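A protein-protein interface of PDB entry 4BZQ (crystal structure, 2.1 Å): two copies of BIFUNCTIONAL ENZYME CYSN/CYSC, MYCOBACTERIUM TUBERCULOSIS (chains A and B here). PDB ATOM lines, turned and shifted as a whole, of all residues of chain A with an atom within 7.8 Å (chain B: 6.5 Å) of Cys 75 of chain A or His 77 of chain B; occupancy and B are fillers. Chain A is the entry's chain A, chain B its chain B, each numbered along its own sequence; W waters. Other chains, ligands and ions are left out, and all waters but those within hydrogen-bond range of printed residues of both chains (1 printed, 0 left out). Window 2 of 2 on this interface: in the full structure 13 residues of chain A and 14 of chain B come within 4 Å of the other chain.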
ATOM      1  N   PRO A   1     -17.288  16.963  -3.877  1.00  0.00           N
ATOM      2  CA  PRO A   1     -15.871  17.374  -3.649  1.00  0.00           C
ATOM      3  C   PRO A   1     -15.420  18.548  -4.530  1.00  0.00           C
ATOM      4  O   PRO A   1     -15.861  18.664  -5.680  1.00  0.00           O
ATOM      5  CB  PRO A   1     -15.063  16.111  -3.983  1.00  0.00           C
ATOM      6  CG  PRO A   1     -16.061  14.984  -4.127  1.00  0.00           C
ATOM      7  CD  PRO A   1     -17.390  15.611  -4.466  1.00  0.00           C
ATOM      8  N   PRO A   2     -14.585  19.440  -3.993  1.00  0.00           N
ATOM      9  CA  PRO A   2     -14.068  20.475  -4.883  1.00  0.00           C
ATOM     10  C   PRO A   2     -13.160  19.832  -5.899  1.00  0.00           C
ATOM     11  O   PRO A   2     -12.602  18.765  -5.664  1.00  0.00           O
ATOM     12  CB  PRO A   2     -13.264  21.375  -3.978  1.00  0.00           C
ATOM     13  CG  PRO A   2     -13.831  21.164  -2.618  1.00  0.00           C
ATOM     14  CD  PRO A   2     -14.338  19.735  -2.582  1.00  0.00           C
ATOM     15  N   ARG A   3     -12.982  20.485  -7.019  1.00  0.00           N
ATOM     16  CA  ARG A   3     -12.242  19.865  -8.117  1.00  0.00           C
ATOM     17  C   ARG A   3     -10.753  19.935  -7.936  1.00  0.00           C
ATOM     18  O   ARG A   3     -10.219  20.856  -7.335  1.00  0.00           O
ATOM     19  CB  ARG A   3     -12.702  20.431  -9.456  1.00  0.00           C
ATOM     20  CG  ARG A   3     -14.017  19.747  -9.835  1.00  0.00           C
ATOM     21  CD  ARG A   3     -14.960  20.588 -10.670  1.00  0.00           C
ATOM     22  NE  ARG A   3     -14.669  20.393 -12.088  1.00  0.00           N
ATOM     23  CZ  ARG A   3     -14.202  21.330 -12.915  1.00  0.00           C
ATOM     24  NH1 ARG A   3     -13.977  22.570 -12.497  1.00  0.00           N
ATOM     25  NH2 ARG A   3     -13.965  21.022 -14.187  1.00  0.00           N
ATOM     26  N   GLY A   4     -10.098  18.901  -8.406  1.00  0.00           N
ATOM     27  CA  GLY A   4      -8.678  18.715  -8.210  1.00  0.00           C
ATOM     28  C   GLY A   4      -7.899  19.583  -9.192  1.00  0.00           C
ATOM     29  O   GLY A   4      -8.461  20.498  -9.833  1.00  0.00           O
ATOM     30  N   SER A  34      -6.017  14.318  -1.035  1.00  0.00           N
ATOM     31  CA  SER A  34      -6.122  13.225  -1.927  1.00  0.00           C
ATOM     32  C   SER A  34      -5.269  13.491  -3.195  1.00  0.00           C
ATOM     33  O   SER A  34      -5.510  14.397  -3.943  1.00  0.00           O
ATOM     34  CB  SER A  34      -7.573  13.037  -2.274  1.00  0.00           C
ATOM     35  OG  SER A  34      -7.655  11.998  -3.226  1.00  0.00           O
ATOM     36  N   VAL A  68      -6.993  11.386 -18.756  1.00  0.00           N
ATOM     37  CA  VAL A  68      -7.158  10.650 -17.520  1.00  0.00           C
ATOM     38  C   VAL A  68      -6.915  11.586 -16.329  1.00  0.00           C
ATOM     39  O   VAL A  68      -7.679  11.615 -15.339  1.00  0.00           O
ATOM     40  CB  VAL A  68      -6.240   9.418 -17.486  1.00  0.00           C
ATOM     41  CG1 VAL A  68      -6.331   8.685 -16.174  1.00  0.00           C
ATOM     42  CG2 VAL A  68      -6.594   8.473 -18.600  1.00  0.00           C
ATOM     43  N   ALA A  69      -5.887  12.400 -16.451  1.00  0.00           N
ATOM     44  CA  ALA A  69      -5.617  13.397 -15.420  1.00  0.00           C
ATOM     45  C   ALA A  69      -6.862  14.269 -15.185  1.00  0.00           C
ATOM     46  O   ALA A  69      -7.265  14.474 -14.030  1.00  0.00           O
ATOM     47  CB  ALA A  69      -4.409  14.265 -15.778  1.00  0.00           C
ATOM     48  N   THR A  70      -7.475  14.791 -16.254  1.00  0.00           N
ATOM     49  CA  THR A  70      -8.608  15.739 -16.050  1.00  0.00           C
ATOM     50  C   THR A  70      -9.748  15.032 -15.399  1.00  0.00           C
ATOM     51  O   THR A  70     -10.538  15.596 -14.630  1.00  0.00           O
ATOM     52  CB  THR A  70      -9.171  16.330 -17.343  1.00  0.00           C
ATOM     53  OG1 THR A  70      -9.595  15.251 -18.134  1.00  0.00           O
ATOM     54  CG2 THR A  70      -8.167  17.078 -18.077  1.00  0.00           C
ATOM     55  N   LEU A  71      -9.851  13.758 -15.689  1.00  0.00           N
ATOM     56  CA  LEU A  71     -10.936  13.026 -15.128  1.00  0.00           C
ATOM     57  C   LEU A  71     -10.730  12.704 -13.692  1.00  0.00           C
ATOM     58  O   LEU A  71     -11.641  12.829 -12.884  1.00  0.00           O
ATOM     59  CB  LEU A  71     -11.078  11.850 -16.014  1.00  0.00           C
ATOM     60  CG  LEU A  71     -11.981  10.704 -15.705  1.00  0.00           C
ATOM     61  CD1 LEU A  71     -12.255  10.042 -17.035  1.00  0.00           C
ATOM     62  CD2 LEU A  71     -11.288   9.758 -14.732  1.00  0.00           C
ATOM     63  N   LEU A  72      -9.520  12.312 -13.325  1.00  0.00           N
ATOM     64  CA  LEU A  72      -9.238  12.169 -11.906  1.00  0.00           C
ATOM     65  C   LEU A  72      -9.296  13.507 -11.153  1.00  0.00           C
ATOM     66  O   LEU A  72      -9.749  13.576 -10.009  1.00  0.00           O
ATOM     67  CB  LEU A  72      -7.924  11.504 -11.702  1.00  0.00           C
ATOM     68  CG  LEU A  72      -7.858  10.070 -12.177  1.00  0.00           C
ATOM     69  CD1 LEU A  72      -6.455   9.562 -11.973  1.00  0.00           C
ATOM     70  CD2 LEU A  72      -8.836   9.154 -11.489  1.00  0.00           C
ATOM     71  N   ALA A  73      -8.862  14.579 -11.799  1.00  0.00           N
ATOM     72  CA  ALA A  73      -8.933  15.918 -11.194  1.00  0.00           C
ATOM     73  C   ALA A  73     -10.391  16.319 -10.927  1.00  0.00           C
ATOM     74  O   ALA A  73     -10.739  16.772  -9.838  1.00  0.00           O
ATOM     75  CB  ALA A  73      -8.267  16.931 -12.065  1.00  0.00           C
ATOM     76  N   ASP A  74     -11.245  16.087 -11.905  1.00  0.00           N
ATOM     77  CA  ASP A  74     -12.658  16.333 -11.747  1.00  0.00           C
ATOM     78  C   ASP A  74     -13.238  15.599 -10.537  1.00  0.00           C
ATOM     79  O   ASP A  74     -14.132  16.092  -9.885  1.00  0.00           O
ATOM     80  CB  ASP A  74     -13.392  15.927 -13.011  1.00  0.00           C
ATOM     81  CG  ASP A  74     -14.825  16.333 -12.973  1.00  0.00           C
ATOM     82  OD1 ASP A  74     -15.076  17.565 -12.958  1.00  0.00           O
ATOM     83  OD2 ASP A  74     -15.690  15.421 -12.913  1.00  0.00           O
ATOM     84  N   CYS A  75     -12.735  14.408 -10.254  1.00  0.00           N
ATOM     85  CA  CYS A  75     -13.132  13.669  -9.060  1.00  0.00           C
ATOM     86  C   CYS A  75     -12.554  14.211  -7.770  1.00  0.00           C
ATOM     87  O   CYS A  75     -12.667  13.552  -6.743  1.00  0.00           O
ATOM     88  CB  CYS A  75     -12.589  12.260  -9.132  1.00  0.00           C
ATOM     89  SG  CYS A  75     -13.398  11.258 -10.316  1.00  0.00           S
ATOM     90  N   GLY A  76     -11.873  15.351  -7.823  1.00  0.00           N
ATOM     91  CA  GLY A  76     -11.288  15.966  -6.633  1.00  0.00           C
ATOM     92  C   GLY A  76      -9.846  15.622  -6.253  1.00  0.00           C
ATOM     93  O   GLY A  76      -9.351  16.085  -5.209  1.00  0.00           O
ATOM     94  N   HIS A  77      -9.139  14.855  -7.081  1.00  0.00           N
ATOM     95  CA  HIS A  77      -7.753  14.538  -6.765  1.00  0.00           C
ATOM     96  C   HIS A  77      -6.758  15.562  -7.261  1.00  0.00           C
ATOM     97  O   HIS A  77      -6.957  16.247  -8.277  1.00  0.00           O
ATOM     98  CB  HIS A  77      -7.367  13.175  -7.332  1.00  0.00           C
ATOM     99  CG  HIS A  77      -8.325  12.099  -6.914  1.00  0.00           C
ATOM    100  ND1 HIS A  77      -8.198  11.392  -5.737  1.00  0.00           N
ATOM    101  CD2 HIS A  77      -9.439  11.628  -7.518  1.00  0.00           C
ATOM    102  CE1 HIS A  77      -9.185  10.517  -5.643  1.00  0.00           C
ATOM    103  NE2 HIS A  77      -9.940  10.636  -6.718  1.00  0.00           N
ATOM    104  N   LEU A  78      -5.637  15.587  -6.566  1.00  0.00           N
ATOM    105  CA  LEU A  78      -4.478  16.316  -7.032  1.00  0.00           C
ATOM    106  C   LEU A  78      -3.628  15.340  -7.816  1.00  0.00           C
ATOM    107  O   LEU A  78      -3.077  14.419  -7.256  1.00  0.00           O
ATOM    108  CB  LEU A  78      -3.742  16.906  -5.834  1.00  0.00           C
ATOM    109  CG  LEU A  78      -2.552  17.814  -6.114  1.00  0.00           C
ATOM    110  CD1 LEU A  78      -1.378  17.117  -6.743  1.00  0.00           C
ATOM    111  CD2 LEU A  78      -2.977  18.968  -6.966  1.00  0.00           C
ATOM    112  N   VAL A  79      -3.568  15.529  -9.128  1.00  0.00           N
ATOM    113  CA  VAL A  79      -2.963  14.586 -10.010  1.00  0.00           C
ATOM    114  C   VAL A  79      -1.499  14.949 -10.336  1.00  0.00           C
ATOM    115  O   VAL A  79      -1.226  16.046 -10.726  1.00  0.00           O
ATOM    116  CB  VAL A  79      -3.812  14.446 -11.277  1.00  0.00           C
ATOM    117  CG1 VAL A  79      -3.223  13.367 -12.214  1.00  0.00           C
ATOM    118  CG2 VAL A  79      -5.274  14.067 -10.927  1.00  0.00           C
ATOM    119  N   ILE A 103      -9.727  22.601 -15.650  1.00  0.00           N
ATOM    120  CA  ILE A 103      -8.894  22.083 -14.552  1.00  0.00           C
ATOM    121  C   ILE A 103      -7.571  22.842 -14.533  1.00  0.00           C
ATOM    122  O   ILE A 103      -6.922  23.011 -15.582  1.00  0.00           O
ATOM    123  CB  ILE A 103      -8.603  20.572 -14.717  1.00  0.00           C
ATOM    124  CG1 ILE A 103      -9.915  19.749 -14.799  1.00  0.00           C
ATOM    125  CG2 ILE A 103      -7.720  20.064 -13.576  1.00  0.00           C
ATOM    126  CD1 ILE A 103     -10.653  19.585 -13.488  1.00  0.00           C
ATOM    127  N   PRO B   2      -9.728   2.868   1.659  1.00  0.00           N
ATOM    128  CA  PRO B   2     -10.014   1.589   0.968  1.00  0.00           C
ATOM    129  C   PRO B   2      -9.781   1.702  -0.569  1.00  0.00           C
ATOM    130  O   PRO B   2     -10.119   2.709  -1.170  1.00  0.00           O
ATOM    131  CB  PRO B   2     -11.496   1.305   1.317  1.00  0.00           C
ATOM    132  CG  PRO B   2     -11.764   2.131   2.534  1.00  0.00           C
ATOM    133  CD  PRO B   2     -10.871   3.345   2.452  1.00  0.00           C
ATOM    134  N   ARG B   3      -9.158   0.716  -1.195  1.00  0.00           N
ATOM    135  CA  ARG B   3      -9.204   0.673  -2.646  1.00  0.00           C
ATOM    136  C   ARG B   3     -10.637   0.376  -3.062  1.00  0.00           C
ATOM    137  O   ARG B   3     -11.371  -0.289  -2.364  1.00  0.00           O
ATOM    138  CB  ARG B   3      -8.298  -0.390  -3.220  1.00  0.00           C
ATOM    139  CG  ARG B   3      -6.887   0.081  -3.375  1.00  0.00           C
ATOM    140  CD  ARG B   3      -6.020  -1.118  -3.651  1.00  0.00           C
ATOM    141  NE  ARG B   3      -5.502  -1.099  -5.006  1.00  0.00           N
ATOM    142  CZ  ARG B   3      -5.130  -2.186  -5.673  1.00  0.00           C
ATOM    143  NH1 ARG B   3      -5.264  -3.399  -5.140  1.00  0.00           N
ATOM    144  NH2 ARG B   3      -4.619  -2.063  -6.882  1.00  0.00           N
ATOM    145  N   GLY B   4     -11.005   0.910  -4.207  1.00  0.00           N
ATOM    146  CA  GLY B   4     -12.338   0.833  -4.730  1.00  0.00           C
ATOM    147  C   GLY B   4     -12.594  -0.508  -5.373  1.00  0.00           C
ATOM    148  O   GLY B   4     -11.832  -1.467  -5.198  1.00  0.00           O
ATOM    149  N   LYS B   5     -13.690  -0.578  -6.118  1.00  0.00           N
ATOM    150  CA  LYS B   5     -14.071  -1.767  -6.913  1.00  0.00           C
ATOM    151  C   LYS B   5     -14.867  -1.357  -8.132  1.00  0.00           C
ATOM    152  O   LYS B   5     -15.339  -0.218  -8.240  1.00  0.00           O
ATOM    153  CB  LYS B   5     -14.904  -2.755  -6.093  1.00  0.00           C
ATOM    154  CG  LYS B   5     -14.484  -2.862  -4.644  1.00  0.00           C
ATOM    155  CD  LYS B   5     -15.473  -3.685  -3.857  1.00  0.00           C
ATOM    156  CE  LYS B   5     -14.956  -3.841  -2.444  1.00  0.00           C
ATOM    157  NZ  LYS B   5     -15.933  -4.680  -1.720  1.00  0.00           N
ATOM    158  N   THR B   6     -15.032  -2.297  -9.040  1.00  0.00           N
ATOM    159  CA  THR B   6     -15.718  -2.024 -10.300  1.00  0.00           C
ATOM    160  C   THR B   6     -16.973  -2.877 -10.556  1.00  0.00           C
ATOM    161  O   THR B   6     -16.956  -4.073 -10.403  1.00  0.00           O
ATOM    162  CB  THR B   6     -14.756  -2.154 -11.494  1.00  0.00           C
ATOM    163  OG1 THR B   6     -13.768  -1.105 -11.413  1.00  0.00           O
ATOM    164  CG2 THR B   6     -15.511  -2.021 -12.833  1.00  0.00           C
ATOM    165  N   SER B  34     -17.923   7.007  -2.273  1.00  0.00           N
ATOM    166  CA  SER B  34     -17.483   7.751  -3.394  1.00  0.00           C
ATOM    167  C   SER B  34     -17.613   6.881  -4.650  1.00  0.00           C
ATOM    168  O   SER B  34     -16.822   6.005  -4.915  1.00  0.00           O
ATOM    169  CB  SER B  34     -16.068   8.231  -3.146  1.00  0.00           C
ATOM    170  OG  SER B  34     -15.694   9.046  -4.242  1.00  0.00           O
ATOM    171  N   ALA B  35     -18.643   7.120  -5.424  1.00  0.00           N
ATOM    172  CA  ALA B  35     -18.940   6.265  -6.548  1.00  0.00           C
ATOM    173  C   ALA B  35     -18.777   7.135  -7.755  1.00  0.00           C
ATOM    174  O   ALA B  35     -18.953   8.332  -7.664  1.00  0.00           O
ATOM    175  CB  ALA B  35     -20.363   5.724  -6.465  1.00  0.00           C
ATOM    176  N   TYR B  36     -18.467   6.523  -8.887  1.00  0.00           N
ATOM    177  CA  TYR B  36     -18.313   7.250 -10.125  1.00  0.00           C
ATOM    178  C   TYR B  36     -18.671   6.410 -11.324  1.00  0.00           C
ATOM    179  O   TYR B  36     -18.302   5.251 -11.452  1.00  0.00           O
ATOM    180  CB  TYR B  36     -16.881   7.684 -10.239  1.00  0.00           C
ATOM    181  CG  TYR B  36     -16.526   8.547 -11.379  1.00  0.00           C
ATOM    182  CD1 TYR B  36     -16.268   8.002 -12.640  1.00  0.00           C
ATOM    183  CD2 TYR B  36     -16.323   9.897 -11.194  1.00  0.00           C
ATOM    184  CE1 TYR B  36     -15.840   8.812 -13.672  1.00  0.00           C
ATOM    185  CE2 TYR B  36     -15.922  10.701 -12.235  1.00  0.00           C
ATOM    186  CZ  TYR B  36     -15.685  10.148 -13.454  1.00  0.00           C
ATOM    187  OH  TYR B  36     -15.273  10.989 -14.468  1.00  0.00           O
ATOM    188  N   ALA B  69     -11.064   2.504 -15.192  1.00  0.00           N
ATOM    189  CA  ALA B  69     -11.788   1.977 -14.037  1.00  0.00           C
ATOM    190  C   ALA B  69     -10.800   1.540 -12.959  1.00  0.00           C
ATOM    191  O   ALA B  69     -10.980   1.876 -11.795  1.00  0.00           O
ATOM    192  CB  ALA B  69     -12.724   0.804 -14.457  1.00  0.00           C
ATOM    193  N   LEU B  71      -7.890   2.489 -12.364  1.00  0.00           N
ATOM    194  CA  LEU B  71      -7.204   3.668 -11.836  1.00  0.00           C
ATOM    195  C   LEU B  71      -8.096   4.450 -10.861  1.00  0.00           C
ATOM    196  O   LEU B  71      -7.657   4.849  -9.754  1.00  0.00           O
ATOM    197  CB  LEU B  71      -6.703   4.578 -12.985  1.00  0.00           C
ATOM    198  CG  LEU B  71      -5.521   4.021 -13.760  1.00  0.00           C
ATOM    199  CD1 LEU B  71      -5.390   4.839 -15.022  1.00  0.00           C
ATOM    200  CD2 LEU B  71      -4.261   4.069 -12.946  1.00  0.00           C
ATOM    201  N   LEU B  72      -9.352   4.672 -11.279  1.00  0.00           N
ATOM    202  CA  LEU B  72     -10.283   5.317 -10.400  1.00  0.00           C
ATOM    203  C   LEU B  72     -10.501   4.410  -9.179  1.00  0.00           C
ATOM    204  O   LEU B  72     -10.626   4.901  -8.064  1.00  0.00           O
ATOM    205  CB  LEU B  72     -11.610   5.628 -11.102  1.00  0.00           C
ATOM    206  CG  LEU B  72     -11.786   6.811 -12.047  1.00  0.00           C
ATOM    207  CD1 LEU B  72     -13.003   6.640 -12.910  1.00  0.00           C
ATOM    208  CD2 LEU B  72     -11.909   8.150 -11.335  1.00  0.00           C
ATOM    209  N   ALA B  73     -10.527   3.092  -9.364  1.00  0.00           N
ATOM    210  CA  ALA B  73     -10.732   2.197  -8.230  1.00  0.00           C
ATOM    211  C   ALA B  73      -9.558   2.295  -7.266  1.00  0.00           C
ATOM    212  O   ALA B  73      -9.730   2.364  -6.048  1.00  0.00           O
ATOM    213  CB  ALA B  73     -10.928   0.759  -8.728  1.00  0.00           C
ATOM    214  N   ASP B  74      -8.352   2.283  -7.802  1.00  0.00           N
ATOM    215  CA  ASP B  74      -7.135   2.454  -6.992  1.00  0.00           C
ATOM    216  C   ASP B  74      -7.148   3.775  -6.198  1.00  0.00           C
ATOM    217  O   ASP B  74      -6.631   3.823  -5.111  1.00  0.00           O
ATOM    218  CB  ASP B  74      -5.923   2.403  -7.932  1.00  0.00           C
ATOM    219  CG  ASP B  74      -4.629   2.208  -7.221  1.00  0.00           C
ATOM    220  OD1 ASP B  74      -4.557   1.361  -6.311  1.00  0.00           O
ATOM    221  OD2 ASP B  74      -3.652   2.852  -7.622  1.00  0.00           O
ATOM    222  N   CYS B  75      -7.785   4.820  -6.721  1.00  0.00           N
ATOM    223  CA  CYS B  75      -7.996   6.067  -5.991  1.00  0.00           C
ATOM    224  C   CYS B  75      -9.088   5.966  -4.959  1.00  0.00           C
ATOM    225  O   CYS B  75      -9.455   6.988  -4.373  1.00  0.00           O
ATOM    226  CB  CYS B  75      -8.498   7.160  -6.912  1.00  0.00           C
ATOM    227  SG  CYS B  75      -7.307   7.857  -7.950  1.00  0.00           S
ATOM    228  N   GLY B  76      -9.664   4.779  -4.771  1.00  0.00           N
ATOM    229  CA  GLY B  76     -10.702   4.590  -3.763  1.00  0.00           C
ATOM    230  C   GLY B  76     -12.161   4.760  -4.194  1.00  0.00           C
ATOM    231  O   GLY B  76     -13.034   4.716  -3.351  1.00  0.00           O
ATOM    232  N   HIS B  77     -12.451   4.926  -5.480  1.00  0.00           N
ATOM    233  CA  HIS B  77     -13.838   5.006  -5.913  1.00  0.00           C
ATOM    234  C   HIS B  77     -14.505   3.637  -6.225  1.00  0.00           C
ATOM    235  O   HIS B  77     -13.863   2.634  -6.579  1.00  0.00           O
ATOM    236  CB  HIS B  77     -13.992   5.832  -7.165  1.00  0.00           C
ATOM    237  CG  HIS B  77     -13.422   7.196  -7.082  1.00  0.00           C
ATOM    238  ND1 HIS B  77     -14.160   8.312  -6.733  1.00  0.00           N
ATOM    239  CD2 HIS B  77     -12.171   7.642  -7.356  1.00  0.00           C
ATOM    240  CE1 HIS B  77     -13.375   9.380  -6.765  1.00  0.00           C
ATOM    241  NE2 HIS B  77     -12.166   8.997  -7.129  1.00  0.00           N
ATOM    242  N   LEU B  78     -15.826   3.627  -6.097  1.00  0.00           N
ATOM    243  CA  LEU B  78     -16.661   2.495  -6.553  1.00  0.00           C
ATOM    244  C   LEU B  78     -17.054   2.859  -7.959  1.00  0.00           C
ATOM    245  O   LEU B  78     -17.816   3.759  -8.175  1.00  0.00           O
ATOM    246  CB  LEU B  78     -17.886   2.304  -5.639  1.00  0.00           C
ATOM    247  CG  LEU B  78     -18.845   1.111  -5.941  1.00  0.00           C
ATOM    248  CD1 LEU B  78     -19.585   1.240  -7.245  1.00  0.00           C
ATOM    249  CD2 LEU B  78     -18.100  -0.197  -5.945  1.00  0.00           C
ATOM    250  N   VAL B  79     -16.501   2.156  -8.916  1.00  0.00           N
ATOM    251  CA  VAL B  79     -16.647   2.521 -10.320  1.00  0.00           C
ATOM    252  C   VAL B  79     -17.789   1.779 -11.010  1.00  0.00           C
ATOM    253  O   VAL B  79     -17.895   0.570 -10.901  1.00  0.00           O
ATOM    254  CB  VAL B  79     -15.325   2.286 -11.067  1.00  0.00           C
ATOM    255  CG1 VAL B  79     -15.418   2.774 -12.513  1.00  0.00           C
ATOM    256  CG2 VAL B  79     -14.184   3.030 -10.365  1.00  0.00           C
HETATM  257  O   HOH W   1     -14.244  13.066 -13.657  1.00  0.00           O
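A ring nitrogen (NE2) of His 77 of chain A lies within hydrogen-bond range of a ring nitrogen (NE2) of His 77 of chain B.
The side-chain hydroxyl (OG) of Ser 34 of chain A sits at hydrogen-bond distance from a ring nitrogen (ND1) of His 77 of chain A, 2.6 Å away. N of Lys 5 of chain B is in hydrogen-bond range of O of His 77 of chain B (3.2 Å). OG of Ser 34 of chain B is in hydrogen-bond range of ND1 of His 77 of chain B (3.0 Å). The backbone NH (N) of Tyr 36 of chain B lies within hydrogen-bond range of the backbone carbonyl oxygen (O) of Leu 78 of chain B. O of Leu 71 of chain B is in hydrogen-bond range of SG of Cys 75 of chain B (3.5 Å). The backbone NH (N) of His 77 of chain B lies within hydrogen-bond range of the backbone carbonyl oxygen (O) of Leu 72 of chain B (3.2 Å).
OH of Tyr 36 of chain B touches CG of Leu 71 of chain A (3.5 Å). CD2 of Leu 71 of chain A touches CD2 of Leu 72 of chain B (3.8 Å). CD2 of Leu 72 of chain A touches CD2 of Leu 72 of chain B, at 3.2 Å. Cys 75 of chain A touches Tyr 36 of chain B. Leu 72 of chain B touches Cys 75 of chain A. CE1 of His 77 of chain B touches CB of Cys 75 of chain A (3.8 Å). CE1 of His 77 of chain A touches CB of Cys 75 of chain B (3.7 Å).
Cys 75 of chain A touches just these residues of chain B: Tyr 36, Leu 72 and His 77. Gly 76 of chain B touches none of the printed residues of chain A. Of the printed residues of chain B, Leu 72 of chain A touches Leu 72. Of the printed residues of chain B, His 77 of chain A touches Cys 75 and His 77. Asp 74 of chain B touches none of the printed residues of chain A. The nearest residue of chain B that does not touch Cys 75 of chain A is Ser 34 of chain B (6.0 Å). The nearest residue of chain A that does not touch His 77 of chain B is Leu 72 of chain A (5.5 Å). The nearest printed residue of chain B that does not touch His 77 of chain A is Leu 72 of chain B (5.6 Å).
Of the 18 printed residues of chain A, 4 touch a printed residue of chain B. Printed residues of chain A that touch a printed residue of chain B: Leu 71, Leu 72, Cys 75 and His 77. Hydrophobic or aromatic side chains of chain A within 4 Å of the printed part of chain B: Leu 71, Leu 72 and His 77. Hydrophobic or aromatic side chains of chain B within 4 Å of the printed part of chain A: Tyr 36, Leu 72 and His 77. Among the printed residues, 8 pairs touch across the chains.
Leu 71 of chain A touches Leu 72 of chain B, but with the chains exchanged Leu 72 of chain A does not touch Leu 71 of chain B (4.8 Å). Leu 72 of chain A touches its own counterpart, Leu 72 of chain B. Cys 75 of chain A touches Leu 72 of chain B, but with the chains exchanged Leu 72 of chain A does not touch Cys 75 of chain B (4.1 Å). Cys 75 of chain A touches His 77 of chain B, and with the chains exchanged His 77 of chain A touches Cys 75 of chain B. Of the 8 pairs that touch across the chains among the printed residues, 4 have their exchanged pair printed and touching as well.
Water W1 lies within hydrogen-bond range of the side-chain hydroxyl of Tyr 36 of chain B (2.5 Å), the backbone carbonyl oxygen of Leu 71 of chain A (2.7 Å) and the side-chain carboxylate of Asp 74 of chain A (2.9 Å).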
